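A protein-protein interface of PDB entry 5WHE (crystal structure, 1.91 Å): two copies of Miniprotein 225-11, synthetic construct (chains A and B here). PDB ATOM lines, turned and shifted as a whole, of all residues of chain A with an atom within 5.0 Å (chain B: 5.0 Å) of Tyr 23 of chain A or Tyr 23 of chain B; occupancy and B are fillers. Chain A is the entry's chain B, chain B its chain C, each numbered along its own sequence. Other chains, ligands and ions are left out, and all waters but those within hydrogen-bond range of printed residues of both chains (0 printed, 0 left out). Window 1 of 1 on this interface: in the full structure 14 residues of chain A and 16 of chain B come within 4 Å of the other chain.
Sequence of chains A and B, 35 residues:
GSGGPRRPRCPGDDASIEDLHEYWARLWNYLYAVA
The side-chain sulfur (SG) of Cys 10 of chain B forms a disulfide with the side-chain sulfur (SG) of Cys 10 of chain A.
OH of Tyr 23 of chain A sits at hydrogen-bond distance from SG of Cys 10 of chain B (3.7 Å).
The backbone carbonyl oxygen (O) of Trp 24 of chain B sits at hydrogen-bond distance from the indole nitrogen (NE1) of Trp 24 of chain A, 3.0 Å away.
SG of Cys 10 of chain A lies close to O of Pro 11 of chain B (3.4 Å).
Tyr 23 of chain A touches just these residues of chain B: Cys 10 (3.7 Å), Tyr 23 (3.3 Å) and Leu 27 (3.8 Å).
Tyr 23 of chain B touches just these residues of chain A: Pro 11 (3.5 Å) and Tyr 23 (3.3 Å).
Printed residues of chain B within 4 Å of Cys 10 of chain A: Cys 10 and Pro 11.
Of the printed residues of chain A, Leu 27 of chain B touches Tyr 23 and Trp 24.
The nearest residue of chain A that does not touch Tyr 23 of chain B is Leu 27 of chain A (4.2 Å).
Of the 14 printed residues of chain A, 6 touch a printed residue of chain B.
Printed residues of chain A that touch a printed residue of chain B: Cys 10, Pro 11, Tyr 23, Trp 24, Leu 27 and Trp 28.
Hydrophobic or aromatic side chains of chain A within 4 Å of the printed part of chain B: Pro 11, Tyr 23, Trp 24, Leu 27 and Trp 28.
Of the 14 printed residues of chain B, 7 touch a printed residue of chain A.
Hydrophobic or aromatic side chains of chain B within 4 Å of the printed part of chain A: Tyr 23, Trp 24, Leu 27 and Trp 28.
Among the printed residues, 13 pairs touch across the chains.
Pro 11 of chain A touches Cys 10 of chain B (CD to SG, 3.8 Å).
Tyr 23 of chain B touches Pro 11 of chain A.
Tyr 23 of chain A touches Tyr 23 of chain B (CE2 to CE2, 3.3 Å).
CD2 of Tyr 23 of chain A touches CD2 of Leu 27 of chain B, at 3.8 Å.
Trp 24 of chain A touches Leu 27 of chain B (CD1 to CB, 3.96 Å).
CZ2 of Trp 24 of chain A touches CD1 of Trp 28 of chain B, 3.4 Å away.
CD2 of Leu 27 of chain A touches O of Leu 20 of chain B (3.6 Å).
CD2 of Leu 27 of chain A touches CB of Trp 24 of chain B (3.6 Å).
Trp 28 of chain A touches Trp 24 of chain B.
Cys 10 of chain B touches its own counterpart, Cys 10 of chain A.
Pro 11 of chain A touches Tyr 23 of chain B, but with the chains exchanged Tyr 23 of chain A does not touch Pro 11 of chain B (5.6 Å).
Trp 24 of chain A touches Trp 28 of chain B, and with the chains exchanged Trp 28 of chain A touches Trp 24 of chain B.
Leu 27 of chain A touches Leu 20 of chain B, but with the chains exchanged Leu 20 of chain A does not touch Leu 27 of chain B (4.1 Å).
14 positions are printed for both chains.
Of the 13 pairs that touch across the chains among the printed residues, 9 have their exchanged pair printed and touching as well.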
ATOM      1  N   PRO A   8      11.839 -19.921  14.547  1.00  0.00           N
ATOM      2  CA  PRO A   8      10.496 -20.251  15.043  1.00  0.00           C
ATOM      3  C   PRO A   8       9.500 -20.468  13.904  1.00  0.00           C
ATOM      4  O   PRO A   8       9.588 -19.779  12.885  1.00  0.00           O
ATOM      5  CB  PRO A   8      10.115 -19.022  15.885  1.00  0.00           C
ATOM      6  CG  PRO A   8      10.982 -17.919  15.380  1.00  0.00           C
ATOM      7  CD  PRO A   8      12.263 -18.565  14.939  1.00  0.00           C
ATOM      8  N   ARG A   9       8.586 -21.423  14.072  1.00  0.00           N
ATOM      9  CA  ARG A   9       7.551 -21.692  13.074  1.00  0.00           C
ATOM     10  C   ARG A   9       6.628 -20.493  12.984  1.00  0.00           C
ATOM     11  O   ARG A   9       6.372 -19.849  14.000  1.00  0.00           O
ATOM     12  CB  ARG A   9       6.749 -22.945  13.440  1.00  0.00           C
ATOM     13  CG  ARG A   9       7.552 -24.242  13.530  1.00  0.00           C
ATOM     14  CD  ARG A   9       6.626 -25.416  13.859  1.00  0.00           C
ATOM     15  NE  ARG A   9       7.304 -26.713  13.878  1.00  0.00           N
ATOM     16  CZ  ARG A   9       6.673 -27.884  13.967  1.00  0.00           C
ATOM     17  NH1 ARG A   9       5.347 -27.922  14.039  1.00  0.00           N
ATOM     18  NH2 ARG A   9       7.362 -29.018  13.978  1.00  0.00           N
ATOM     19  N   CYS A  10       6.125 -20.188  11.787  1.00  0.00           N
ATOM     20  CA  CYS A  10       5.175 -19.086  11.631  1.00  0.00           C
ATOM     21  C   CYS A  10       4.005 -19.283  12.597  1.00  0.00           C
ATOM     22  O   CYS A  10       3.634 -20.418  12.897  1.00  0.00           O
ATOM     23  CB  CYS A  10       4.683 -18.978  10.180  1.00  0.00           C
ATOM     24  SG  CYS A  10       5.807 -18.056   9.072  1.00  0.00           S
ATOM     25  N   PRO A  11       3.451 -18.177  13.118  1.00  0.00           N
ATOM     26  CA  PRO A  11       2.458 -18.251  14.201  1.00  0.00           C
ATOM     27  C   PRO A  11       1.153 -18.940  13.821  1.00  0.00           C
ATOM     28  O   PRO A  11       0.469 -19.485  14.692  1.00  0.00           O
ATOM     29  CB  PRO A  11       2.200 -16.778  14.546  1.00  0.00           C
ATOM     30  CG  PRO A  11       2.727 -15.990  13.388  1.00  0.00           C
ATOM     31  CD  PRO A  11       3.845 -16.791  12.818  1.00  0.00           C
ATOM     32  N   ASP A  19      -0.691 -15.163  20.876  1.00  0.00           N
ATOM     33  CA  ASP A  19       0.138 -16.064  20.069  1.00  0.00           C
ATOM     34  C   ASP A  19       1.199 -15.303  19.279  1.00  0.00           C
ATOM     35  O   ASP A  19       2.326 -15.772  19.132  1.00  0.00           O
ATOM     36  CB  ASP A  19      -0.710 -16.882  19.090  1.00  0.00           C
ATOM     37  CG  ASP A  19      -1.632 -17.880  19.787  1.00  0.00           C
ATOM     38  OD1 ASP A  19      -1.377 -18.237  20.955  1.00  0.00           O
ATOM     39  OD2 ASP A  19      -2.607 -18.320  19.140  1.00  0.00           O
ATOM     40  N   LEU A  20       0.828 -14.142  18.757  1.00  0.00           N
ATOM     41  CA  LEU A  20       1.776 -13.311  18.016  1.00  0.00           C
ATOM     42  C   LEU A  20       2.843 -12.743  18.949  1.00  0.00           C
ATOM     43  O   LEU A  20       4.012 -12.653  18.572  1.00  0.00           O
ATOM     44  CB  LEU A  20       1.056 -12.175  17.283  1.00  0.00           C
ATOM     45  CG  LEU A  20       0.126 -12.528  16.112  1.00  0.00           C
ATOM     46  CD1 LEU A  20      -0.453 -11.271  15.471  1.00  0.00           C
ATOM     47  CD2 LEU A  20       0.839 -13.373  15.068  1.00  0.00           C
ATOM     48  N   HIS A  21       2.443 -12.355  20.159  1.00  0.00           N
ATOM     49  CA  HIS A  21       3.406 -11.873  21.143  1.00  0.00           C
ATOM     50  C   HIS A  21       4.420 -12.962  21.471  1.00  0.00           C
ATOM     51  O   HIS A  21       5.621 -12.695  21.568  1.00  0.00           O
ATOM     52  CB  HIS A  21       2.710 -11.415  22.421  1.00  0.00           C
ATOM     53  CG  HIS A  21       2.222  -9.998  22.376  1.00  0.00           C
ATOM     54  ND1 HIS A  21       3.071  -8.926  22.498  1.00  0.00           N
ATOM     55  CD2 HIS A  21       0.977  -9.495  22.243  1.00  0.00           C
ATOM     56  CE1 HIS A  21       2.364  -7.804  22.432  1.00  0.00           C
ATOM     57  NE2 HIS A  21       1.092  -8.123  22.283  1.00  0.00           N
ATOM     58  N   GLU A  22       3.936 -14.187  21.640  1.00  0.00           N
ATOM     59  CA  GLU A  22       4.813 -15.317  21.927  1.00  0.00           C
ATOM     60  C   GLU A  22       5.806 -15.530  20.777  1.00  0.00           C
ATOM     61  O   GLU A  22       7.015 -15.721  21.003  1.00  0.00           O
ATOM     62  CB  GLU A  22       3.987 -16.594  22.183  1.00  0.00           C
ATOM     63  CG  GLU A  22       3.365 -16.689  23.589  1.00  0.00           C
ATOM     64  CD  GLU A  22       4.353 -17.175  24.659  1.00  0.00           C
ATOM     65  OE1 GLU A  22       5.477 -17.591  24.309  1.00  0.00           O
ATOM     66  OE2 GLU A  22       4.004 -17.146  25.858  1.00  0.00           O
ATOM     67  N   TYR A  23       5.297 -15.500  19.548  1.00  0.00           N
ATOM     68  CA  TYR A  23       6.148 -15.693  18.377  1.00  0.00           C
ATOM     69  C   TYR A  23       7.184 -14.586  18.292  1.00  0.00           C
ATOM     70  O   TYR A  23       8.359 -14.858  18.041  1.00  0.00           O
ATOM     71  CB  TYR A  23       5.327 -15.738  17.069  1.00  0.00           C
ATOM     72  CG  TYR A  23       6.193 -15.647  15.832  1.00  0.00           C
ATOM     73  CD1 TYR A  23       6.749 -16.785  15.265  1.00  0.00           C
ATOM     74  CD2 TYR A  23       6.478 -14.420  15.246  1.00  0.00           C
ATOM     75  CE1 TYR A  23       7.562 -16.705  14.139  1.00  0.00           C
ATOM     76  CE2 TYR A  23       7.291 -14.327  14.133  1.00  0.00           C
ATOM     77  CZ  TYR A  23       7.824 -15.473  13.579  1.00  0.00           C
ATOM     78  OH  TYR A  23       8.622 -15.385  12.462  1.00  0.00           O
ATOM     79  N   TRP A  24       6.744 -13.345  18.511  1.00  0.00           N
ATOM     80  CA  TRP A  24       7.622 -12.190  18.362  1.00  0.00           C
ATOM     81  C   TRP A  24       8.828 -12.289  19.299  1.00  0.00           C
ATOM     82  O   TRP A  24       9.954 -11.998  18.898  1.00  0.00           O
ATOM     83  CB  TRP A  24       6.871 -10.883  18.612  1.00  0.00           C
ATOM     84  CG  TRP A  24       7.721  -9.680  18.340  1.00  0.00           C
ATOM     85  CD1 TRP A  24       7.892  -9.049  17.135  1.00  0.00           C
ATOM     86  CD2 TRP A  24       8.528  -8.966  19.284  1.00  0.00           C
ATOM     87  NE1 TRP A  24       8.762  -7.989  17.275  1.00  0.00           N
ATOM     88  CE2 TRP A  24       9.163  -7.916  18.585  1.00  0.00           C
ATOM     89  CE3 TRP A  24       8.783  -9.118  20.651  1.00  0.00           C
ATOM     90  CZ2 TRP A  24      10.032  -7.021  19.208  1.00  0.00           C
ATOM     91  CZ3 TRP A  24       9.646  -8.230  21.267  1.00  0.00           C
ATOM     92  CH2 TRP A  24      10.259  -7.193  20.549  1.00  0.00           C
ATOM     93  N   ALA A  25       8.601 -12.714  20.535  1.00  0.00           N
ATOM     94  CA  ALA A  25       9.702 -12.853  21.489  1.00  0.00           C
ATOM     95  C   ALA A  25      10.688 -13.933  21.026  1.00  0.00           C
ATOM     96  O   ALA A  25      11.907 -13.786  21.170  1.00  0.00           O
ATOM     97  CB  ALA A  25       9.161 -13.170  22.892  1.00  0.00           C
ATOM     98  N   ARG A  26      10.159 -15.013  20.462  1.00  0.00           N
ATOM     99  CA  ARG A  26      10.994 -16.063  19.895  1.00  0.00           C
ATOM    100  C   ARG A  26      11.844 -15.540  18.737  1.00  0.00           C
ATOM    101  O   ARG A  26      13.048 -15.808  18.665  1.00  0.00           O
ATOM    102  CB  ARG A  26      10.128 -17.242  19.423  1.00  0.00           C
ATOM    103  CG  ARG A  26       9.410 -17.967  20.564  1.00  0.00           C
ATOM    104  CD  ARG A  26       8.881 -19.325  20.131  1.00  0.00           C
ATOM    105  NE  ARG A  26       8.407 -20.096  21.280  1.00  0.00           N
ATOM    106  CZ  ARG A  26       7.131 -20.226  21.626  1.00  0.00           C
ATOM    107  NH1 ARG A  26       6.180 -19.647  20.905  1.00  0.00           N
ATOM    108  NH2 ARG A  26       6.806 -20.943  22.693  1.00  0.00           N
ATOM    109  N   LEU A  27      11.216 -14.788  17.838  1.00  0.00           N
ATOM    110  CA  LEU A  27      11.914 -14.264  16.664  1.00  0.00           C
ATOM    111  C   LEU A  27      12.984 -13.251  17.048  1.00  0.00           C
ATOM    112  O   LEU A  27      14.068 -13.235  16.461  1.00  0.00           O
ATOM    113  CB  LEU A  27      10.924 -13.622  15.684  1.00  0.00           C
ATOM    114  CG  LEU A  27      11.501 -13.088  14.366  1.00  0.00           C
ATOM    115  CD1 LEU A  27      12.103 -14.218  13.532  1.00  0.00           C
ATOM    116  CD2 LEU A  27      10.438 -12.351  13.567  1.00  0.00           C
ATOM    117  N   TRP A  28      12.651 -12.390  18.006  1.00  0.00           N
ATOM    118  CA  TRP A  28      13.580 -11.410  18.582  1.00  0.00           C
ATOM    119  C   TRP A  28      14.888 -12.093  18.992  1.00  0.00           C
ATOM    120  O   TRP A  28      15.976 -11.656  18.626  1.00  0.00           O
ATOM    121  CB  TRP A  28      12.909 -10.746  19.774  1.00  0.00           C
ATOM    122  CG  TRP A  28      13.550  -9.544  20.409  1.00  0.00           C
ATOM    123  CD1 TRP A  28      14.367  -8.621  19.822  1.00  0.00           C
ATOM    124  CD2 TRP A  28      13.366  -9.119  21.764  1.00  0.00           C
ATOM    125  NE1 TRP A  28      14.714  -7.651  20.737  1.00  0.00           N
ATOM    126  CE2 TRP A  28      14.111  -7.935  21.939  1.00  0.00           C
ATOM    127  CE3 TRP A  28      12.640  -9.622  22.850  1.00  0.00           C
ATOM    128  CZ2 TRP A  28      14.153  -7.249  23.154  1.00  0.00           C
ATOM    129  CZ3 TRP A  28      12.683  -8.945  24.060  1.00  0.00           C
ATOM    130  CH2 TRP A  28      13.438  -7.769  24.204  1.00  0.00           C
ATOM    131  N   PRO B   8       0.736  -7.934   9.632  1.00  0.00           N
ATOM    132  CA  PRO B   8       1.761  -8.378   8.686  1.00  0.00           C
ATOM    133  C   PRO B   8       1.705  -9.889   8.475  1.00  0.00           C
ATOM    134  O   PRO B   8       1.234 -10.616   9.349  1.00  0.00           O
ATOM    135  CB  PRO B   8       3.072  -7.955   9.363  1.00  0.00           C
ATOM    136  CG  PRO B   8       2.726  -7.900  10.828  1.00  0.00           C
ATOM    137  CD  PRO B   8       1.313  -7.427  10.892  1.00  0.00           C
ATOM    138  N   ARG B   9       2.169 -10.351   7.318  1.00  0.00           N
ATOM    139  CA  ARG B   9       2.198 -11.781   7.017  1.00  0.00           C
ATOM    140  C   ARG B   9       3.571 -12.396   7.253  1.00  0.00           C
ATOM    141  O   ARG B   9       4.592 -11.825   6.862  1.00  0.00           O
ATOM    142  CB  ARG B   9       1.783 -12.030   5.569  1.00  0.00           C
ATOM    143  CG  ARG B   9       0.351 -11.663   5.250  1.00  0.00           C
ATOM    144  CD  ARG B   9       0.063 -11.965   3.789  1.00  0.00           C
ATOM    145  NE  ARG B   9      -1.330 -11.723   3.425  1.00  0.00           N
ATOM    146  CZ  ARG B   9      -1.807 -11.867   2.192  1.00  0.00           C
ATOM    147  NH1 ARG B   9      -0.999 -12.248   1.213  1.00  0.00           N
ATOM    148  NH2 ARG B   9      -3.088 -11.628   1.937  1.00  0.00           N
ATOM    149  N   CYS B  10       3.591 -13.577   7.863  1.00  0.00           N
ATOM    150  CA  CYS B  10       4.842 -14.281   8.140  1.00  0.00           C
ATOM    151  C   CYS B  10       5.441 -14.861   6.860  1.00  0.00           C
ATOM    152  O   CYS B  10       4.784 -15.636   6.168  1.00  0.00           O
ATOM    153  CB  CYS B  10       4.610 -15.393   9.168  1.00  0.00           C
ATOM    154  SG  CYS B  10       6.127 -16.181   9.800  1.00  0.00           S
ATOM    155  N   PRO B  11       6.691 -14.485   6.532  1.00  0.00           N
ATOM    156  CA  PRO B  11       7.276 -14.969   5.273  1.00  0.00           C
ATOM    157  C   PRO B  11       7.558 -16.467   5.303  1.00  0.00           C
ATOM    158  O   PRO B  11       7.636 -17.051   6.376  1.00  0.00           O
ATOM    159  CB  PRO B  11       8.571 -14.157   5.146  1.00  0.00           C
ATOM    160  CG  PRO B  11       8.899 -13.732   6.520  1.00  0.00           C
ATOM    161  CD  PRO B  11       7.591 -13.566   7.248  1.00  0.00           C
ATOM    162  N   ASP B  19      14.263 -10.485   5.466  1.00  0.00           N
ATOM    163  CA  ASP B  19      12.799 -10.622   5.396  1.00  0.00           C
ATOM    164  C   ASP B  19      12.223 -10.841   6.792  1.00  0.00           C
ATOM    165  O   ASP B  19      11.189 -10.267   7.141  1.00  0.00           O
ATOM    166  CB  ASP B  19      12.378 -11.783   4.498  1.00  0.00           C
ATOM    167  CG  ASP B  19      12.734 -11.567   3.037  1.00  0.00           C
ATOM    168  OD1 ASP B  19      12.639 -10.422   2.545  1.00  0.00           O
ATOM    169  OD2 ASP B  19      13.096 -12.566   2.382  1.00  0.00           O
ATOM    170  N   LEU B  20      12.890 -11.681   7.580  1.00  0.00           N
ATOM    171  CA  LEU B  20      12.429 -11.972   8.937  1.00  0.00           C
ATOM    172  C   LEU B  20      12.565 -10.746   9.835  1.00  0.00           C
ATOM    173  O   LEU B  20      11.751 -10.527  10.727  1.00  0.00           O
ATOM    174  CB  LEU B  20      13.199 -13.152   9.529  1.00  0.00           C
ATOM    175  CG  LEU B  20      12.772 -14.527   9.007  1.00  0.00           C
ATOM    176  CD1 LEU B  20      13.640 -15.618   9.609  1.00  0.00           C
ATOM    177  CD2 LEU B  20      11.288 -14.787   9.309  1.00  0.00           C
ATOM    178  N   HIS B  21      13.598  -9.949   9.586  1.00  0.00           N
ATOM    179  CA  HIS B  21      13.789  -8.696  10.302  1.00  0.00           C
ATOM    180  C   HIS B  21      12.658  -7.719  10.019  1.00  0.00           C
ATOM    181  O   HIS B  21      12.168  -7.032  10.912  1.00  0.00           O
ATOM    182  CB  HIS B  21      15.127  -8.054   9.917  1.00  0.00           C
ATOM    183  CG  HIS B  21      15.406  -6.776  10.640  1.00  0.00           C
ATOM    184  ND1 HIS B  21      15.983  -6.742  11.895  1.00  0.00           N
ATOM    185  CD2 HIS B  21      15.166  -5.489  10.302  1.00  0.00           C
ATOM    186  CE1 HIS B  21      16.097  -5.487  12.289  1.00  0.00           C
ATOM    187  NE2 HIS B  21      15.608  -4.707  11.342  1.00  0.00           N
ATOM    188  N   GLU B  22      12.269  -7.644   8.755  1.00  0.00           N
ATOM    189  CA  GLU B  22      11.189  -6.764   8.345  1.00  0.00           C
ATOM    190  C   GLU B  22       9.881  -7.182   9.022  1.00  0.00           C
ATOM    191  O   GLU B  22       9.116  -6.346   9.481  1.00  0.00           O
ATOM    192  CB  GLU B  22      11.044  -6.783   6.818  1.00  0.00           C
ATOM    193  CG  GLU B  22      12.221  -6.155   6.065  1.00  0.00           C
ATOM    194  CD  GLU B  22      12.327  -6.651   4.635  1.00  0.00           C
ATOM    195  OE1 GLU B  22      13.345  -6.342   3.967  1.00  0.00           O
ATOM    196  OE2 GLU B  22      11.397  -7.353   4.179  1.00  0.00           O
ATOM    197  N   TYR B  23       9.650  -8.486   9.084  1.00  0.00           N
ATOM    198  CA  TYR B  23       8.455  -9.023   9.716  1.00  0.00           C
ATOM    199  C   TYR B  23       8.475  -8.772  11.225  1.00  0.00           C
ATOM    200  O   TYR B  23       7.454  -8.433  11.826  1.00  0.00           O
ATOM    201  CB  TYR B  23       8.335 -10.512   9.403  1.00  0.00           C
ATOM    202  CG  TYR B  23       7.157 -11.195  10.051  1.00  0.00           C
ATOM    203  CD1 TYR B  23       5.878 -10.660   9.964  1.00  0.00           C
ATOM    204  CD2 TYR B  23       7.319 -12.398  10.721  1.00  0.00           C
ATOM    205  CE1 TYR B  23       4.789 -11.300  10.557  1.00  0.00           C
ATOM    206  CE2 TYR B  23       6.246 -13.042  11.309  1.00  0.00           C
ATOM    207  CZ  TYR B  23       4.983 -12.494  11.227  1.00  0.00           C
ATOM    208  OH  TYR B  23       3.919 -13.149  11.825  1.00  0.00           O
ATOM    209  N   TRP B  24       9.650  -8.918  11.822  1.00  0.00           N
ATOM    210  CA  TRP B  24       9.871  -8.575  13.220  1.00  0.00           C
ATOM    211  C   TRP B  24       9.494  -7.122  13.512  1.00  0.00           C
ATOM    212  O   TRP B  24       8.834  -6.822  14.514  1.00  0.00           O
ATOM    213  CB  TRP B  24      11.337  -8.822  13.577  1.00  0.00           C
ATOM    214  CG  TRP B  24      11.719  -8.377  14.953  1.00  0.00           C
ATOM    215  CD1 TRP B  24      11.581  -9.090  16.113  1.00  0.00           C
ATOM    216  CD2 TRP B  24      12.315  -7.121  15.319  1.00  0.00           C
ATOM    217  NE1 TRP B  24      12.044  -8.351  17.174  1.00  0.00           N
ATOM    218  CE2 TRP B  24      12.500  -7.136  16.716  1.00  0.00           C
ATOM    219  CE3 TRP B  24      12.687  -5.975  14.600  1.00  0.00           C
ATOM    220  CZ2 TRP B  24      13.054  -6.057  17.415  1.00  0.00           C
ATOM    221  CZ3 TRP B  24      13.237  -4.901  15.286  1.00  0.00           C
ATOM    222  CH2 TRP B  24      13.419  -4.951  16.684  1.00  0.00           C
ATOM    223  N   ALA B  25       9.911  -6.223  12.625  1.00  0.00           N
ATOM    224  CA  ALA B  25       9.668  -4.797  12.793  1.00  0.00           C
ATOM    225  C   ALA B  25       8.204  -4.442  12.551  1.00  0.00           C
ATOM    226  O   ALA B  25       7.625  -3.636  13.280  1.00  0.00           O
ATOM    227  CB  ALA B  25      10.562  -3.990  11.857  1.00  0.00           C
ATOM    228  N   ARG B  26       7.609  -5.038  11.525  1.00  0.00           N
ATOM    229  CA  ARG B  26       6.219  -4.757  11.203  1.00  0.00           C
ATOM    230  C   ARG B  26       5.304  -5.324  12.290  1.00  0.00           C
ATOM    231  O   ARG B  26       4.276  -4.743  12.617  1.00  0.00           O
ATOM    232  CB  ARG B  26       5.843  -5.340   9.839  1.00  0.00           C
ATOM    233  CG  ARG B  26       6.607  -4.745   8.680  1.00  0.00           C
ATOM    234  CD  ARG B  26       6.143  -5.346   7.362  1.00  0.00           C
ATOM    235  NE  ARG B  26       7.119  -5.147   6.292  1.00  0.00           N
ATOM    236  CZ  ARG B  26       7.252  -4.023   5.591  1.00  0.00           C
ATOM    237  NH1 ARG B  26       6.471  -2.979   5.842  1.00  0.00           N
ATOM    238  NH2 ARG B  26       8.169  -3.941   4.638  1.00  0.00           N
ATOM    239  N   LEU B  27       5.697  -6.464  12.836  1.00  0.00           N
ATOM    240  CA  LEU B  27       4.924  -7.111  13.887  1.00  0.00           C
ATOM    241  C   LEU B  27       5.014  -6.315  15.187  1.00  0.00           C
ATOM    242  O   LEU B  27       4.021  -6.188  15.898  1.00  0.00           O
ATOM    243  CB  LEU B  27       5.412  -8.544  14.091  1.00  0.00           C
ATOM    244  CG  LEU B  27       4.559  -9.567  14.837  1.00  0.00           C
ATOM    245  CD1 LEU B  27       3.113  -9.558  14.363  1.00  0.00           C
ATOM    246  CD2 LEU B  27       5.177 -10.939  14.630  1.00  0.00           C
ATOM    247  N   TRP B  28       6.200  -5.788  15.495  1.00  0.00           N
ATOM    248  CA  TRP B  28       6.363  -4.899  16.648  1.00  0.00           C
ATOM    249  C   TRP B  28       5.403  -3.727  16.518  1.00  0.00           C
ATOM    250  O   TRP B  28       4.716  -3.364  17.473  1.00  0.00           O
ATOM    251  CB  TRP B  28       7.804  -4.386  16.771  1.00  0.00           C
ATOM    252  CG  TRP B  28       8.010  -3.559  18.005  1.00  0.00           C
ATOM    253  CD1 TRP B  28       8.433  -4.000  19.223  1.00  0.00           C
ATOM    254  CD2 TRP B  28       7.762  -2.152  18.152  1.00  0.00           C
ATOM    255  NE1 TRP B  28       8.475  -2.958  20.115  1.00  0.00           N
ATOM    256  CE2 TRP B  28       8.070  -1.814  19.484  1.00  0.00           C
ATOM    257  CE3 TRP B  28       7.312  -1.148  17.287  1.00  0.00           C
ATOM    258  CZ2 TRP B  28       7.943  -0.514  19.971  1.00  0.00           C
ATOM    259  CZ3 TRP B  28       7.189   0.143  17.775  1.00  0.00           C
ATOM    260  CH2 TRP B  28       7.503   0.447  19.104  1.00  0.00           C
